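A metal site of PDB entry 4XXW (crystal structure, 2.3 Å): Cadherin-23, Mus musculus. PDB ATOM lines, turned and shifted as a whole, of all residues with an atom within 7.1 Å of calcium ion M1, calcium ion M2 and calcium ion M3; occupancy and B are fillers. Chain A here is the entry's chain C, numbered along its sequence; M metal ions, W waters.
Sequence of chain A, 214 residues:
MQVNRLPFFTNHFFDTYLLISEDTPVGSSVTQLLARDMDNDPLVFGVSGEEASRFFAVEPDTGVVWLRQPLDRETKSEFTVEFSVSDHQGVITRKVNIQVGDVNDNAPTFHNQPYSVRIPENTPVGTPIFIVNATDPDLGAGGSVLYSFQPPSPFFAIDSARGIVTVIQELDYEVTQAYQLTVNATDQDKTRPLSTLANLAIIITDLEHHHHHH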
ATOM      1  N   GLU A  22       2.411  23.389  -0.313  1.00  0.00           N
ATOM      2  CA  GLU A  22       1.058  24.003  -0.186  1.00  0.00           C
ATOM      3  C   GLU A  22       0.893  25.353  -0.861  1.00  0.00           C
ATOM      4  O   GLU A  22      -0.177  25.791  -0.995  1.00  0.00           O
ATOM      5  CB  GLU A  22       0.581  24.183   1.279  1.00  0.00           C
ATOM      6  CG  GLU A  22       1.458  25.068   2.140  1.00  0.00           C
ATOM      7  CD  GLU A  22       0.835  25.413   3.516  1.00  0.00           C
ATOM      8  OE1 GLU A  22      -0.374  25.472   3.570  1.00  0.00           O
ATOM      9  OE2 GLU A  22       1.529  25.613   4.527  1.00  0.00           O
ATOM     10  N   LEU A  71      -4.156  23.511  -1.837  1.00  0.00           N
ATOM     11  CA  LEU A  71      -3.681  22.639  -0.770  1.00  0.00           C
ATOM     12  C   LEU A  71      -3.514  23.477   0.487  1.00  0.00           C
ATOM     13  O   LEU A  71      -3.324  24.665   0.396  1.00  0.00           O
ATOM     14  CB  LEU A  71      -2.344  22.014  -1.134  1.00  0.00           C
ATOM     15  CG  LEU A  71      -2.351  21.079  -2.328  1.00  0.00           C
ATOM     16  CD1 LEU A  71      -0.997  20.441  -2.669  1.00  0.00           C
ATOM     17  CD2 LEU A  71      -3.386  19.984  -2.100  1.00  0.00           C
ATOM     18  N   ASP A  72      -3.647  22.865   1.651  1.00  0.00           N
ATOM     19  CA  ASP A  72      -3.406  23.580   2.920  1.00  0.00           C
ATOM     20  C   ASP A  72      -2.718  22.638   3.891  1.00  0.00           C
ATOM     21  O   ASP A  72      -3.365  21.788   4.451  1.00  0.00           O
ATOM     22  CB  ASP A  72      -4.718  24.112   3.561  1.00  0.00           C
ATOM     23  CG  ASP A  72      -4.429  24.961   4.837  1.00  0.00           C
ATOM     24  OD1 ASP A  72      -3.233  25.352   5.060  1.00  0.00           O
ATOM     25  OD2 ASP A  72      -5.370  25.241   5.643  1.00  0.00           O
ATOM     26  N   ARG A  73      -1.423  22.781   4.112  1.00  0.00           N
ATOM     27  CA  ARG A  73      -0.718  21.799   4.985  1.00  0.00           C
ATOM     28  C   ARG A  73      -1.334  21.707   6.418  1.00  0.00           C
ATOM     29  O   ARG A  73      -1.384  20.635   7.000  1.00  0.00           O
ATOM     30  CB  ARG A  73       0.776  22.121   4.978  1.00  0.00           C
ATOM     31  CG  ARG A  73       1.765  21.020   5.363  1.00  0.00           C
ATOM     32  CD  ARG A  73       1.690  20.583   6.819  1.00  0.00           C
ATOM     33  NE  ARG A  73       1.628  21.739   7.727  1.00  0.00           N
ATOM     34  CZ  ARG A  73       1.422  21.670   9.035  1.00  0.00           C
ATOM     35  NH1 ARG A  73       1.240  20.506   9.646  1.00  0.00           N
ATOM     36  NH2 ARG A  73       1.441  22.779   9.750  1.00  0.00           N
ATOM     37  N   GLU A  74      -1.867  22.825   6.912  1.00  0.00           N
ATOM     38  CA  GLU A  74      -2.493  22.940   8.242  1.00  0.00           C
ATOM     39  C   GLU A  74      -3.805  22.182   8.372  1.00  0.00           C
ATOM     40  O   GLU A  74      -4.212  21.907   9.488  1.00  0.00           O
ATOM     41  CB  GLU A  74      -2.765  24.426   8.617  1.00  0.00           C
ATOM     42  CG  GLU A  74      -1.522  25.208   9.056  1.00  0.00           C
ATOM     43  CD  GLU A  74      -0.384  25.371   8.013  1.00  0.00           C
ATOM     44  OE1 GLU A  74      -0.603  25.803   6.863  1.00  0.00           O
ATOM     45  OE2 GLU A  74       0.796  25.164   8.352  1.00  0.00           O
ATOM     46  N   THR A  75      -4.471  21.890   7.284  1.00  0.00           N
ATOM     47  CA  THR A  75      -5.668  21.099   7.275  1.00  0.00           C
ATOM     48  C   THR A  75      -5.422  19.646   6.940  1.00  0.00           C
ATOM     49  O   THR A  75      -5.947  18.754   7.588  1.00  0.00           O
ATOM     50  CB  THR A  75      -6.702  21.689   6.273  1.00  0.00           C
ATOM     51  OG1 THR A  75      -6.997  23.027   6.644  1.00  0.00           O
ATOM     52  CG2 THR A  75      -8.032  20.918   6.260  1.00  0.00           C
ATOM     53  N   GLY A 101       3.827  19.799   1.321  1.00  0.00           N
ATOM     54  CA  GLY A 101       4.948  20.523   1.918  1.00  0.00           C
ATOM     55  C   GLY A 101       4.490  21.804   2.650  1.00  0.00           C
ATOM     56  O   GLY A 101       3.561  22.523   2.221  1.00  0.00           O
ATOM     57  N   ASP A 102       5.091  22.075   3.775  1.00  0.00           N
ATOM     58  CA  ASP A 102       4.676  23.247   4.558  1.00  0.00           C
ATOM     59  C   ASP A 102       5.391  24.490   4.068  1.00  0.00           C
ATOM     60  O   ASP A 102       6.583  24.461   3.786  1.00  0.00           O
ATOM     61  CB  ASP A 102       4.960  23.059   6.044  1.00  0.00           C
ATOM     62  CG  ASP A 102       4.276  24.148   6.893  1.00  0.00           C
ATOM     63  OD1 ASP A 102       3.055  24.274   6.783  1.00  0.00           O
ATOM     64  OD2 ASP A 102       4.968  24.901   7.665  1.00  0.00           O
ATOM     65  N   VAL A 103       4.640  25.605   4.024  1.00  0.00           N
ATOM     66  CA  VAL A 103       5.325  26.930   4.002  1.00  0.00           C
ATOM     67  C   VAL A 103       4.899  27.697   5.189  1.00  0.00           C
ATOM     68  O   VAL A 103       3.850  27.432   5.778  1.00  0.00           O
ATOM     69  CB  VAL A 103       5.145  27.755   2.685  1.00  0.00           C
ATOM     70  CG1 VAL A 103       5.471  26.882   1.486  1.00  0.00           C
ATOM     71  CG2 VAL A 103       3.721  28.257   2.527  1.00  0.00           C
ATOM     72  N   ASN A 104       5.730  28.675   5.516  1.00  0.00           N
ATOM     73  CA  ASN A 104       5.373  29.609   6.528  1.00  0.00           C
ATOM     74  C   ASN A 104       4.303  30.622   6.091  1.00  0.00           C
ATOM     75  O   ASN A 104       4.621  31.722   5.619  1.00  0.00           O
ATOM     76  CB  ASN A 104       6.554  30.374   7.160  1.00  0.00           C
ATOM     77  CG  ASN A 104       6.084  31.082   8.491  1.00  0.00           C
ATOM     78  OD1 ASN A 104       5.355  30.502   9.225  1.00  0.00           O
ATOM     79  ND2 ASN A 104       6.574  32.285   8.769  1.00  0.00           N
ATOM     80  N   ASP A 105       3.051  30.287   6.354  1.00  0.00           N
ATOM     81  CA  ASP A 105       1.934  31.075   5.895  1.00  0.00           C
ATOM     82  C   ASP A 105       0.989  31.539   6.981  1.00  0.00           C
ATOM     83  O   ASP A 105      -0.046  32.039   6.645  1.00  0.00           O
ATOM     84  CB  ASP A 105       1.148  30.400   4.690  1.00  0.00           C
ATOM     85  CG  ASP A 105       0.484  29.032   5.041  1.00  0.00           C
ATOM     86  OD1 ASP A 105       0.723  28.398   6.103  1.00  0.00           O
ATOM     87  OD2 ASP A 105      -0.305  28.539   4.193  1.00  0.00           O
ATOM     88  N   ASN A 106       1.331  31.359   8.238  1.00  0.00           N
ATOM     89  CA  ASN A 106       0.545  31.839   9.338  1.00  0.00           C
ATOM     90  C   ASN A 106       1.408  32.692  10.297  1.00  0.00           C
ATOM     91  O   ASN A 106       2.551  32.338  10.645  1.00  0.00           O
ATOM     92  CB  ASN A 106      -0.050  30.661  10.117  1.00  0.00           C
ATOM     93  CG  ASN A 106      -1.010  29.828   9.305  1.00  0.00           C
ATOM     94  OD1 ASN A 106      -0.582  28.948   8.478  1.00  0.00           O
ATOM     95  ND2 ASN A 106      -2.257  29.966   9.598  1.00  0.00           N
ATOM     96  N   ALA A 107       0.837  33.829  10.682  1.00  0.00           N
ATOM     97  CA  ALA A 107       1.431  34.628  11.751  1.00  0.00           C
ATOM     98  C   ALA A 107       0.946  34.055  13.068  1.00  0.00           C
ATOM     99  O   ALA A 107      -0.076  33.389  13.077  1.00  0.00           O
ATOM    100  CB  ALA A 107       1.048  36.067  11.583  1.00  0.00           C
ATOM    101  N   PRO A 108       1.683  34.255  14.161  1.00  0.00           N
ATOM    102  CA  PRO A 108       1.263  33.865  15.466  1.00  0.00           C
ATOM    103  C   PRO A 108      -0.108  34.495  15.819  1.00  0.00           C
ATOM    104  O   PRO A 108      -0.428  35.600  15.338  1.00  0.00           O
ATOM    105  CB  PRO A 108       2.309  34.460  16.352  1.00  0.00           C
ATOM    106  CG  PRO A 108       3.548  34.430  15.535  1.00  0.00           C
ATOM    107  CD  PRO A 108       3.049  34.848  14.196  1.00  0.00           C
ATOM    108  N   ASP A 136       1.013  29.168  16.816  1.00  0.00           N
ATOM    109  CA  ASP A 136       1.403  29.325  15.370  1.00  0.00           C
ATOM    110  C   ASP A 136       1.510  27.919  14.817  1.00  0.00           C
ATOM    111  O   ASP A 136       2.306  27.076  15.310  1.00  0.00           O
ATOM    112  CB  ASP A 136       2.655  30.174  15.186  1.00  0.00           C
ATOM    113  CG  ASP A 136       3.039  30.466  13.635  1.00  0.00           C
ATOM    114  OD1 ASP A 136       2.868  29.568  12.724  1.00  0.00           O
ATOM    115  OD2 ASP A 136       3.560  31.609  13.382  1.00  0.00           O
ATOM    116  N   PRO A 137       0.626  27.604  13.879  1.00  0.00           N
ATOM    117  CA  PRO A 137       0.425  26.240  13.470  1.00  0.00           C
ATOM    118  C   PRO A 137       1.352  25.802  12.312  1.00  0.00           C
ATOM    119  O   PRO A 137       1.308  24.686  11.942  1.00  0.00           O
ATOM    120  CB  PRO A 137      -1.036  26.262  12.981  1.00  0.00           C
ATOM    121  CG  PRO A 137      -1.151  27.643  12.375  1.00  0.00           C
ATOM    122  CD  PRO A 137      -0.379  28.531  13.298  1.00  0.00           C
ATOM    123  N   ASP A 138       2.222  26.637  11.801  1.00  0.00           N
ATOM    124  CA  ASP A 138       3.201  26.166  10.804  1.00  0.00           C
ATOM    125  C   ASP A 138       4.183  25.200  11.425  1.00  0.00           C
ATOM    126  O   ASP A 138       4.303  25.127  12.607  1.00  0.00           O
ATOM    127  CB  ASP A 138       3.962  27.304  10.182  1.00  0.00           C
ATOM    128  CG  ASP A 138       3.038  28.273   9.488  1.00  0.00           C
ATOM    129  OD1 ASP A 138       2.407  27.841   8.493  1.00  0.00           O
ATOM    130  OD2 ASP A 138       2.928  29.448   9.994  1.00  0.00           O
ATOM    131  N   LEU A 139       4.831  24.430  10.564  1.00  0.00           N
ATOM    132  CA  LEU A 139       5.846  23.486  11.018  1.00  0.00           C
ATOM    133  C   LEU A 139       7.101  24.173  11.485  1.00  0.00           C
ATOM    134  O   LEU A 139       7.539  25.187  10.888  1.00  0.00           O
ATOM    135  CB  LEU A 139       6.143  22.430   9.984  1.00  0.00           C
ATOM    136  CG  LEU A 139       5.005  21.381   9.834  1.00  0.00           C
ATOM    137  CD1 LEU A 139       5.443  20.165   9.038  1.00  0.00           C
ATOM    138  CD2 LEU A 139       4.438  20.881  11.138  1.00  0.00           C
ATOM    139  N   ALA A 141      10.431  25.665  12.858  1.00  0.00           N
ATOM    140  CA  ALA A 141      10.837  27.030  13.230  1.00  0.00           C
ATOM    141  C   ALA A 141       9.750  28.033  12.883  1.00  0.00           C
ATOM    142  O   ALA A 141       9.538  28.994  13.611  1.00  0.00           O
ATOM    143  CB  ALA A 141      12.116  27.396  12.479  1.00  0.00           C
ATOM    144  N   GLY A 142       9.063  27.775  11.765  1.00  0.00           N
ATOM    145  CA  GLY A 142       7.913  28.516  11.366  1.00  0.00           C
ATOM    146  C   GLY A 142       6.716  28.586  12.337  1.00  0.00           C
ATOM    147  O   GLY A 142       5.805  29.426  12.160  1.00  0.00           O
ATOM    148  N   GLY A 143       6.670  27.664  13.291  1.00  0.00           N
ATOM    149  CA  GLY A 143       5.598  27.564  14.263  1.00  0.00           C
ATOM    150  C   GLY A 143       6.063  27.765  15.673  1.00  0.00           C
ATOM    151  O   GLY A 143       5.267  27.544  16.569  1.00  0.00           O
ATOM    152  N   SER A 144       7.313  28.168  15.879  1.00  0.00           N
ATOM    153  CA  SER A 144       7.947  28.337  17.197  1.00  0.00           C
ATOM    154  C   SER A 144       7.982  29.849  17.544  1.00  0.00           C
ATOM    155  O   SER A 144       8.675  30.624  16.896  1.00  0.00           O
ATOM    156  CB  SER A 144       9.397  27.818  17.108  1.00  0.00           C
ATOM    157  OG  SER A 144      10.090  27.950  18.346  1.00  0.00           O
ATOM    158  N   THR A 186       6.650  36.613  17.268  1.00  0.00           N
ATOM    159  CA  THR A 186       7.130  36.247  15.928  1.00  0.00           C
ATOM    160  C   THR A 186       7.423  34.789  15.853  1.00  0.00           C
ATOM    161  O   THR A 186       7.862  34.188  16.822  1.00  0.00           O
ATOM    162  CB  THR A 186       8.402  37.018  15.546  1.00  0.00           C
ATOM    163  OG1 THR A 186       8.763  36.680  14.217  1.00  0.00           O
ATOM    164  CG2 THR A 186       9.641  36.753  16.493  1.00  0.00           C
ATOM    165  N   ASP A 187       7.158  34.175  14.711  1.00  0.00           N
ATOM    166  CA  ASP A 187       7.727  32.863  14.458  1.00  0.00           C
ATOM    167  C   ASP A 187       9.203  33.027  14.050  1.00  0.00           C
ATOM    168  O   ASP A 187       9.674  34.173  13.955  1.00  0.00           O
ATOM    169  CB  ASP A 187       6.875  32.069  13.473  1.00  0.00           C
ATOM    170  CG  ASP A 187       6.880  32.618  12.026  1.00  0.00           C
ATOM    171  OD1 ASP A 187       7.970  33.075  11.537  1.00  0.00           O
ATOM    172  OD2 ASP A 187       5.767  32.531  11.390  1.00  0.00           O
ATOM    173  N   GLN A 188       9.903  31.896  13.847  1.00  0.00           N
ATOM    174  CA  GLN A 188      11.312  31.904  13.600  1.00  0.00           C
ATOM    175  C   GLN A 188      11.696  31.371  12.249  1.00  0.00           C
ATOM    176  O   GLN A 188      12.750  30.843  12.081  1.00  0.00           O
ATOM    177  CB  GLN A 188      12.022  31.118  14.682  1.00  0.00           C
ATOM    178  CG  GLN A 188      11.870  31.808  16.036  1.00  0.00           C
ATOM    179  CD  GLN A 188      12.434  30.973  17.139  1.00  0.00           C
ATOM    180  OE1 GLN A 188      11.718  30.162  17.735  1.00  0.00           O
ATOM    181  NE2 GLN A 188      13.732  31.085  17.352  1.00  0.00           N
ATOM    182  N   ASP A 189      10.830  31.520  11.263  1.00  0.00           N
ATOM    183  CA  ASP A 189      11.130  31.007   9.997  1.00  0.00           C
ATOM    184  C   ASP A 189      12.417  31.700   9.473  1.00  0.00           C
ATOM    185  O   ASP A 189      12.597  32.893   9.586  1.00  0.00           O
ATOM    186  CB  ASP A 189       9.961  31.161   9.040  1.00  0.00           C
ATOM    187  CG  ASP A 189      10.287  30.617   7.669  1.00  0.00           C
ATOM    188  OD1 ASP A 189      10.032  29.437   7.463  1.00  0.00           O
ATOM    189  OD2 ASP A 189      10.731  31.375   6.806  1.00  0.00           O
ATOM    190  N   ARG A 192      11.378  33.893   5.968  1.00  0.00           N
ATOM    191  CA  ARG A 192      10.132  34.647   5.937  1.00  0.00           C
ATOM    192  C   ARG A 192       9.395  34.607   7.282  1.00  0.00           C
ATOM    193  O   ARG A 192       8.325  34.097   7.382  1.00  0.00           O
ATOM    194  CB  ARG A 192       9.228  34.221   4.789  1.00  0.00           C
ATOM    195  CG  ARG A 192       9.835  34.303   3.362  1.00  0.00           C
ATOM    196  CD  ARG A 192       8.927  33.612   2.295  1.00  0.00           C
ATOM    197  NE  ARG A 192       7.690  34.378   2.179  1.00  0.00           N
ATOM    198  CZ  ARG A 192       6.539  34.137   2.830  1.00  0.00           C
ATOM    199  NH1 ARG A 192       6.360  33.009   3.548  1.00  0.00           N
ATOM    200  NH2 ARG A 192       5.534  35.029   2.752  1.00  0.00           N
ATOM    201  N   PRO A 193       9.993  35.174   8.312  1.00  0.00           N
ATOM    202  CA  PRO A 193       9.337  35.184   9.573  1.00  0.00           C
ATOM    203  C   PRO A 193       8.086  36.073   9.501  1.00  0.00           C
ATOM    204  O   PRO A 193       8.033  37.043   8.780  1.00  0.00           O
ATOM    205  CB  PRO A 193      10.407  35.744  10.525  1.00  0.00           C
ATOM    206  CG  PRO A 193      11.298  36.576   9.697  1.00  0.00           C
ATOM    207  CD  PRO A 193      11.291  35.888   8.357  1.00  0.00           C
ATOM    208  N   LEU A 194       7.086  35.714  10.270  1.00  0.00           N
ATOM    209  CA  LEU A 194       5.869  36.451  10.369  1.00  0.00           C
ATOM    210  C   LEU A 194       5.636  36.735  11.858  1.00  0.00           C
ATOM    211  O   LEU A 194       5.862  35.906  12.731  1.00  0.00           O
ATOM    212  CB  LEU A 194       4.718  35.589   9.802  1.00  0.00           C
ATOM    213  CG  LEU A 194       4.832  35.395   8.268  1.00  0.00           C
ATOM    214  CD1 LEU A 194       3.766  34.415   7.835  1.00  0.00           C
ATOM    215  CD2 LEU A 194       4.670  36.706   7.508  1.00  0.00           C
HETATM  216 CA    CA M   1      -1.554  26.770   5.016  1.00  0.00          CA
HETATM  217 CA    CA M   2       1.938  26.397   6.687  1.00  0.00          CA
HETATM  218 CA    CA M   3       4.252  30.872  11.196  1.00  0.00          CA
HETATM  219  O   HOH W   1      -2.787  27.421   2.961  1.00  0.00           O
HETATM  220  O   HOH W   2      -2.777  28.280   6.661  1.00  0.00           O
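Calcium ion M3 is bound by the side-chain carboxylate (OD2) of Asp 187 (2.3 Å), the side-chain carboxylate (OD2) of Asp 138 (2.3 Å), the side-chain amide oxygen (OD1) of Asn 104 (2.3 Å), the backbone carbonyl oxygen (O) of Asn 106 (2.3 Å), the backbone carbonyl oxygen (O) of Gly 142 (2.3 Å), the side-chain carboxylate (OD2) of Asp 136 (2.4 Å) and the side-chain carboxylate (OD1) of Asp 136 (2.4 Å).
Of the 29 residues printed, 6 come within 4 Å of calcium ion M3.
Along chain A the residues within 4 Å of calcium ion M3 span positions 104 to 187.
Calcium ion M2 is bound by OE2 of Glu 22 (2.3 Å), O of Val 103 (2.4 Å), OD1 of Asp 138 (2.4 Å), OE2 of Glu 74 (2.4 Å), OD1 of Asp 102 (2.4 Å), OD1 of Asp 105 (2.4 Å) and OE1 of Glu 74 (2.6 Å).
Calcium ion M1 is bound by the side-chain carboxylate of Asp 72 (2.2 Å), the side-chain carboxylate of Glu 22 (2.3 Å), the side-chain carboxylate of Glu 74 (2.3 Å), the side-chain carboxylate of Asp 105 (2.3 Å), water W1 (2.5 Å) and water W2 (2.5 Å).
Slightly farther from calcium ion M1 lies the side-chain carboxylate (OD1) of Asp 105 (3.0 Å).
Of the 29 residues printed, 4 come within 4 Å of calcium ion M1.
The nearest printed residue that does not touch calcium ion M1 is Arg 73 (4.1 Å).
The side-chain hydroxyl (OG1) of Thr 75 is in hydrogen-bond range of the side-chain carboxylate (OD2) of Asp 72, at 2.9 Å.
O of Leu 194 is in hydrogen-bond range of N of Asp 187, 2.9 Å away.
The backbone NH (N) of Asp 189 is in hydrogen-bond range of the side-chain carboxylate (OD1) of Asp 187 (3.3 Å).
The backbone NH (N) of Glu 22 sits at hydrogen-bond distance from the backbone carbonyl oxygen (O) of Gly 101 (2.9 Å).
The backbone carbonyl oxygen (O) of Arg 192 is in hydrogen-bond range of the side-chain amide nitrogen (ND2) of Asn 104 (2.9 Å).
The side-chain carboxylate (OE2) of Glu 74 lies close to the guanidinium group (NH2) of Arg 73.
The side-chain amide oxygen (OD1) of Asn 106 sits close to the side-chain carboxylate (OD1) of Asp 105.
The side-chain carboxylate (OD2) of Asp 102 sits at hydrogen-bond distance from the backbone NH (N) of Leu 139 (2.9 Å).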
